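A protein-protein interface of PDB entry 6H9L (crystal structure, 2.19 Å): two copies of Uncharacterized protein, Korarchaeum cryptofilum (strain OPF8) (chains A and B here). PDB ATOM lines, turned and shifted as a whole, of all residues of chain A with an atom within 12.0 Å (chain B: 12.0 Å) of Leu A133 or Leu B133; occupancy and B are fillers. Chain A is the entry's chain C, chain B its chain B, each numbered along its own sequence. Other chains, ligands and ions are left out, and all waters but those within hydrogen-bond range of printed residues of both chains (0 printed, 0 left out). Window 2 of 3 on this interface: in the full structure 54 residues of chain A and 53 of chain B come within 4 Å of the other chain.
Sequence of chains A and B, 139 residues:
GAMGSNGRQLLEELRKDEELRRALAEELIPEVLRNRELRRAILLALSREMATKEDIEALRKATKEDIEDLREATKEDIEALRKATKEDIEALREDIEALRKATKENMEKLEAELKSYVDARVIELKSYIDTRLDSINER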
ATOM      1  N   ILE A 123     -26.228   5.608  21.126  1.00  0.00           N
ATOM      2  CA  ILE A 123     -26.494   4.174  20.991  1.00  0.00           C
ATOM      3  C   ILE A 123     -25.183   3.390  21.060  1.00  0.00           C
ATOM      4  O   ILE A 123     -25.122   2.314  21.657  1.00  0.00           O
ATOM      5  CB  ILE A 123     -27.219   3.852  19.665  1.00  0.00           C
ATOM      6  CG1 ILE A 123     -28.618   4.476  19.657  1.00  0.00           C
ATOM      7  CG2 ILE A 123     -27.337   2.344  19.453  1.00  0.00           C
ATOM      8  CD1 ILE A 123     -29.227   4.579  18.276  1.00  0.00           C
ATOM      9  N   GLU A 124     -24.143   3.945  20.447  1.00  0.00           N
ATOM     10  CA  GLU A 124     -22.816   3.338  20.445  1.00  0.00           C
ATOM     11  C   GLU A 124     -22.258   3.211  21.862  1.00  0.00           C
ATOM     12  O   GLU A 124     -21.721   2.167  22.232  1.00  0.00           O
ATOM     13  CB  GLU A 124     -21.869   4.170  19.582  1.00  0.00           C
ATOM     14  CG  GLU A 124     -20.591   3.460  19.178  1.00  0.00           C
ATOM     15  CD  GLU A 124     -19.806   4.236  18.136  1.00  0.00           C
ATOM     16  OE1 GLU A 124     -18.593   3.977  17.989  1.00  0.00           O
ATOM     17  OE2 GLU A 124     -20.399   5.105  17.465  1.00  0.00           O
ATOM     18  N   LEU A 125     -22.393   4.278  22.646  1.00  0.00           N
ATOM     19  CA  LEU A 125     -21.939   4.280  24.037  1.00  0.00           C
ATOM     20  C   LEU A 125     -22.775   3.363  24.922  1.00  0.00           C
ATOM     21  O   LEU A 125     -22.225   2.635  25.743  1.00  0.00           O
ATOM     22  CB  LEU A 125     -21.945   5.698  24.622  1.00  0.00           C
ATOM     23  CG  LEU A 125     -20.665   6.519  24.449  1.00  0.00           C
ATOM     24  CD1 LEU A 125     -20.910   7.958  24.866  1.00  0.00           C
ATOM     25  CD2 LEU A 125     -19.506   5.931  25.243  1.00  0.00           C
ATOM     26  N   LYS A 126     -24.096   3.414  24.766  1.00  0.00           N
ATOM     27  CA  LYS A 126     -24.994   2.567  25.561  1.00  0.00           C
ATOM     28  C   LYS A 126     -24.690   1.087  25.330  1.00  0.00           C
ATOM     29  O   LYS A 126     -24.640   0.302  26.274  1.00  0.00           O
ATOM     30  CB  LYS A 126     -26.464   2.856  25.251  1.00  0.00           C
ATOM     31  CG  LYS A 126     -27.391   2.489  26.399  1.00  0.00           C
ATOM     32  CD  LYS A 126     -28.859   2.570  26.034  1.00  0.00           C
ATOM     33  CE  LYS A 126     -29.719   1.760  26.994  1.00  0.00           C
ATOM     34  NZ  LYS A 126     -29.572   0.282  26.849  1.00  0.00           N
ATOM     35  N   SER A 127     -24.479   0.723  24.068  1.00  0.00           N
ATOM     36  CA  SER A 127     -24.064  -0.627  23.700  1.00  0.00           C
ATOM     37  C   SER A 127     -22.721  -1.003  24.340  1.00  0.00           C
ATOM     38  O   SER A 127     -22.554  -2.116  24.837  1.00  0.00           O
ATOM     39  CB  SER A 127     -23.973  -0.742  22.175  1.00  0.00           C
ATOM     40  OG  SER A 127     -23.563  -2.037  21.772  1.00  0.00           O
ATOM     41  N   TYR A 128     -21.771  -0.069  24.327  1.00  0.00           N
ATOM     42  CA  TYR A 128     -20.452  -0.285  24.934  1.00  0.00           C
ATOM     43  C   TYR A 128     -20.534  -0.460  26.453  1.00  0.00           C
ATOM     44  O   TYR A 128     -19.849  -1.311  27.023  1.00  0.00           O
ATOM     45  CB  TYR A 128     -19.514   0.879  24.597  1.00  0.00           C
ATOM     46  CG  TYR A 128     -18.161   0.807  25.270  1.00  0.00           C
ATOM     47  CD1 TYR A 128     -17.165  -0.042  24.790  1.00  0.00           C
ATOM     48  CD2 TYR A 128     -17.872   1.593  26.385  1.00  0.00           C
ATOM     49  CE1 TYR A 128     -15.925  -0.112  25.402  1.00  0.00           C
ATOM     50  CE2 TYR A 128     -16.632   1.529  27.002  1.00  0.00           C
ATOM     51  CZ  TYR A 128     -15.663   0.677  26.507  1.00  0.00           C
ATOM     52  OH  TYR A 128     -14.432   0.613  27.115  1.00  0.00           O
ATOM     53  N   ILE A 129     -21.363   0.356  27.099  1.00  0.00           N
ATOM     54  CA  ILE A 129     -21.607   0.245  28.539  1.00  0.00           C
ATOM     55  C   ILE A 129     -22.182  -1.125  28.861  1.00  0.00           C
ATOM     56  O   ILE A 129     -21.668  -1.829  29.726  1.00  0.00           O
ATOM     57  CB  ILE A 129     -22.598   1.320  29.037  1.00  0.00           C
ATOM     58  CG1 ILE A 129     -21.965   2.711  28.954  1.00  0.00           C
ATOM     59  CG2 ILE A 129     -23.026   1.054  30.475  1.00  0.00           C
ATOM     60  CD1 ILE A 129     -22.978   3.826  28.819  1.00  0.00           C
ATOM     61  N   ASP A 130     -23.249  -1.484  28.151  1.00  0.00           N
ATOM     62  CA  ASP A 130     -23.943  -2.755  28.355  1.00  0.00           C
ATOM     63  C   ASP A 130     -23.032  -3.964  28.161  1.00  0.00           C
ATOM     64  O   ASP A 130     -23.150  -4.948  28.898  1.00  0.00           O
ATOM     65  CB  ASP A 130     -25.134  -2.880  27.401  1.00  0.00           C
ATOM     66  CG  ASP A 130     -26.261  -1.916  27.732  1.00  0.00           C
ATOM     67  OD1 ASP A 130     -26.156  -1.180  28.736  1.00  0.00           O
ATOM     68  OD2 ASP A 130     -27.255  -1.891  26.978  1.00  0.00           O
ATOM     69  N   THR A 131     -22.144  -3.889  27.165  1.00  0.00           N
ATOM     70  CA  THR A 131     -21.220  -4.986  26.840  1.00  0.00           C
ATOM     71  C   THR A 131     -20.248  -5.204  28.009  1.00  0.00           C
ATOM     72  O   THR A 131     -19.930  -6.343  28.369  1.00  0.00           O
ATOM     73  CB  THR A 131     -20.459  -4.737  25.483  1.00  0.00           C
ATOM     74  OG1 THR A 131     -20.420  -5.938  24.700  1.00  0.00           O
ATOM     75  CG2 THR A 131     -19.014  -4.227  25.678  1.00  0.00           C
ATOM     76  N   ARG A 132     -19.796  -4.098  28.600  1.00  0.00           N
ATOM     77  CA  ARG A 132     -18.956  -4.131  29.793  1.00  0.00           C
ATOM     78  C   ARG A 132     -19.697  -4.734  30.991  1.00  0.00           C
ATOM     79  O   ARG A 132     -19.198  -5.671  31.619  1.00  0.00           O
ATOM     80  CB  ARG A 132     -18.465  -2.724  30.137  1.00  0.00           C
ATOM     81  N   LEU A 133     -20.882  -4.205  31.296  1.00  0.00           N
ATOM     82  CA  LEU A 133     -21.684  -4.704  32.422  1.00  0.00           C
ATOM     83  C   LEU A 133     -22.861  -5.555  31.944  1.00  0.00           C
ATOM     84  O   LEU A 133     -22.865  -6.779  32.107  1.00  0.00           O
ATOM     85  CB  LEU A 133     -22.158  -3.556  33.334  1.00  0.00           C
ATOM     86  CG  LEU A 133     -22.815  -2.283  32.780  1.00  0.00           C
ATOM     87  CD1 LEU A 133     -24.210  -2.544  32.223  1.00  0.00           C
ATOM     88  CD2 LEU A 133     -22.883  -1.220  33.865  1.00  0.00           C
ATOM     89  N   GLU B 124     -27.929  11.987  30.802  1.00  0.00           N
ATOM     90  CA  GLU B 124     -28.788  10.812  30.709  1.00  0.00           C
ATOM     91  C   GLU B 124     -27.972   9.523  30.763  1.00  0.00           C
ATOM     92  O   GLU B 124     -28.331   8.586  31.478  1.00  0.00           O
ATOM     93  CB  GLU B 124     -29.592  10.863  29.413  1.00  0.00           C
ATOM     94  CG  GLU B 124     -30.779   9.918  29.362  1.00  0.00           C
ATOM     95  CD  GLU B 124     -31.652  10.154  28.143  1.00  0.00           C
ATOM     96  OE1 GLU B 124     -32.421   9.242  27.777  1.00  0.00           O
ATOM     97  OE2 GLU B 124     -31.571  11.247  27.544  1.00  0.00           O
ATOM     98  N   LEU B 125     -26.873   9.489  30.012  1.00  0.00           N
ATOM     99  CA  LEU B 125     -25.977   8.331  29.999  1.00  0.00           C
ATOM    100  C   LEU B 125     -25.236   8.156  31.320  1.00  0.00           C
ATOM    101  O   LEU B 125     -25.125   7.041  31.821  1.00  0.00           O
ATOM    102  CB  LEU B 125     -24.961   8.424  28.855  1.00  0.00           C
ATOM    103  CG  LEU B 125     -25.380   7.820  27.515  1.00  0.00           C
ATOM    104  CD1 LEU B 125     -24.374   8.198  26.440  1.00  0.00           C
ATOM    105  CD2 LEU B 125     -25.514   6.305  27.597  1.00  0.00           C
ATOM    106  N   LYS B 126     -24.722   9.250  31.872  1.00  0.00           N
ATOM    107  CA  LYS B 126     -24.011   9.206  33.153  1.00  0.00           C
ATOM    108  C   LYS B 126     -24.909   8.658  34.261  1.00  0.00           C
ATOM    109  O   LYS B 126     -24.482   7.827  35.061  1.00  0.00           O
ATOM    110  CB  LYS B 126     -23.500  10.599  33.537  1.00  0.00           C
ATOM    111  N   SER B 127     -26.150   9.133  34.297  1.00  0.00           N
ATOM    112  CA  SER B 127     -27.159   8.631  35.226  1.00  0.00           C
ATOM    113  C   SER B 127     -27.428   7.132  35.014  1.00  0.00           C
ATOM    114  O   SER B 127     -27.543   6.377  35.976  1.00  0.00           O
ATOM    115  CB  SER B 127     -28.455   9.426  35.057  1.00  0.00           C
ATOM    116  OG  SER B 127     -29.472   8.966  35.924  1.00  0.00           O
ATOM    117  N   TYR B 128     -27.517   6.711  33.752  1.00  0.00           N
ATOM    118  CA  TYR B 128     -27.729   5.299  33.406  1.00  0.00           C
ATOM    119  C   TYR B 128     -26.555   4.414  33.830  1.00  0.00           C
ATOM    120  O   TYR B 128     -26.756   3.310  34.332  1.00  0.00           O
ATOM    121  CB  TYR B 128     -27.978   5.150  31.898  1.00  0.00           C
ATOM    122  CG  TYR B 128     -28.095   3.720  31.416  1.00  0.00           C
ATOM    123  CD1 TYR B 128     -29.268   2.996  31.603  1.00  0.00           C
ATOM    124  CD2 TYR B 128     -27.037   3.094  30.761  1.00  0.00           C
ATOM    125  CE1 TYR B 128     -29.385   1.689  31.155  1.00  0.00           C
ATOM    126  CE2 TYR B 128     -27.141   1.788  30.313  1.00  0.00           C
ATOM    127  CZ  TYR B 128     -28.319   1.092  30.511  1.00  0.00           C
ATOM    128  OH  TYR B 128     -28.428  -0.201  30.065  1.00  0.00           O
ATOM    129  N   ILE B 129     -25.336   4.901  33.608  1.00  0.00           N
ATOM    130  CA  ILE B 129     -24.124   4.201  34.031  1.00  0.00           C
ATOM    131  C   ILE B 129     -24.131   4.029  35.540  1.00  0.00           C
ATOM    132  O   ILE B 129     -23.962   2.923  36.042  1.00  0.00           O
ATOM    133  CB  ILE B 129     -22.851   4.977  33.634  1.00  0.00           C
ATOM    134  CG1 ILE B 129     -22.671   4.977  32.114  1.00  0.00           C
ATOM    135  CG2 ILE B 129     -21.611   4.367  34.276  1.00  0.00           C
ATOM    136  CD1 ILE B 129     -21.874   6.156  31.598  1.00  0.00           C
ATOM    137  N   ASP B 130     -24.333   5.139  36.246  1.00  0.00           N
ATOM    138  CA  ASP B 130     -24.330   5.162  37.709  1.00  0.00           C
ATOM    139  C   ASP B 130     -25.374   4.237  38.313  1.00  0.00           C
ATOM    140  O   ASP B 130     -25.121   3.588  39.333  1.00  0.00           O
ATOM    141  CB  ASP B 130     -24.586   6.579  38.230  1.00  0.00           C
ATOM    142  CG  ASP B 130     -23.427   7.522  37.965  1.00  0.00           C
ATOM    143  OD1 ASP B 130     -22.392   7.076  37.426  1.00  0.00           O
ATOM    144  OD2 ASP B 130     -23.556   8.718  38.299  1.00  0.00           O
ATOM    145  N   THR B 131     -26.549   4.193  37.694  1.00  0.00           N
ATOM    146  CA  THR B 131     -27.646   3.380  38.205  1.00  0.00           C
ATOM    147  C   THR B 131     -27.336   1.895  38.082  1.00  0.00           C
ATOM    148  O   THR B 131     -27.666   1.117  38.976  1.00  0.00           O
ATOM    149  CB  THR B 131     -28.953   3.691  37.480  1.00  0.00           C
ATOM    150  OG1 THR B 131     -29.264   5.075  37.665  1.00  0.00           O
ATOM    151  CG2 THR B 131     -30.092   2.830  38.012  1.00  0.00           C
ATOM    152  N   ARG B 132     -26.700   1.512  36.978  1.00  0.00           N
ATOM    153  CA  ARG B 132     -26.283   0.133  36.772  1.00  0.00           C
ATOM    154  C   ARG B 132     -25.293  -0.262  37.862  1.00  0.00           C
ATOM    155  O   ARG B 132     -25.389  -1.351  38.425  1.00  0.00           O
ATOM    156  CB  ARG B 132     -25.653  -0.042  35.387  1.00  0.00           C
ATOM    157  N   LEU B 133     -24.367   0.643  38.170  1.00  0.00           N
ATOM    158  CA  LEU B 133     -23.373   0.424  39.217  1.00  0.00           C
ATOM    159  C   LEU B 133     -23.895   0.916  40.562  1.00  0.00           C
ATOM    160  O   LEU B 133     -24.755   0.284  41.176  1.00  0.00           O
ATOM    161  CB  LEU B 133     -22.070   1.147  38.868  1.00  0.00           C
ATOM    162  CG  LEU B 133     -21.494   0.885  37.471  1.00  0.00           C
ATOM    163  CD1 LEU B 133     -20.245   1.724  37.249  1.00  0.00           C
ATOM    164  CD2 LEU B 133     -21.192  -0.590  37.254  1.00  0.00           C
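The side-chain amino group of Lys A126 lies within salt-bridge range of the side-chain carboxylate of Asp A130.
CD1 of Leu A125 touches CD1 of Leu B125 (3.8 Å).
Leu B125 touches Ile A129 (CD2 to CD1, 3.8 Å).
Ile A129 touches Ile B129.
Leu A133 touches Arg B132.
Leu A133 touches Leu B133 (CD2 to CD2, 3.8 Å).
Printed residues of chain B within 4 Å of Leu A125: Leu B125 (3.8 Å).
Ile A129 touches just these residues of chain B: Leu B125 and Ile B129.
Of the printed residues of chain B, Asp A130 touches Tyr B128.
Arg A132 touches none of the printed residues of chain B.
Printed residues of chain B within 4 Å of Leu A133: Arg B132 and Leu B133.
Printed residues of chain A within 4 Å of Leu B125: Leu A125 and Ile A129.
No residue of chain A comes within 4 Å of Thr B131.
Of chain A, only Leu A133 (3.4 Å) comes within 4 Å of Arg B132.
Of chain A, only Leu A133 (3.8 Å) comes within 4 Å of Leu B133.
The nearest residue of chain B that does not touch Leu A133 is Ile B129 (4.8 Å).
The nearest residue of chain A that does not touch Leu B133 is Ile A129 (7.2 Å).
The nearest printed residue of chain B that does not touch Leu A125 is Tyr B128 (6.8 Å).
The side-chain amino group of Lys A126 is in hydrogen-bond range of the side-chain hydroxyl of Tyr B128 (3.4 Å).
The side-chain carboxylate of Asp A130 is in hydrogen-bond range of the side-chain hydroxyl of Tyr B128 (2.8 Å).
Lys A126 touches Tyr B128, but with the chains exchanged Tyr A128 does not touch Lys B126 (11.6 Å).
Ile A129 touches Leu B125, but with the chains exchanged Leu A125 does not touch Ile B129 (6.8 Å).
Ile A129 touches its own counterpart, Ile B129.
Leu A133 touches Arg B132, but with the chains exchanged Arg A132 does not touch Leu B133 (7.7 Å).
Positions printed for both chains: 124, 125, 126, 127, 128, 129, 130, 131, 132 and 133.
Hydrophobic or aromatic side chains of chain A within 4 Å of the printed part of chain B: Leu A125, Ile A129 and Leu A133.
Along chain A the printed residues that touch a printed residue of chain B span positions 125 to 133.
Among the printed residues, no Asp or Glu carboxylate lies within 4 Å of a Lys or Arg side-chain nitrogen of the other chain.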
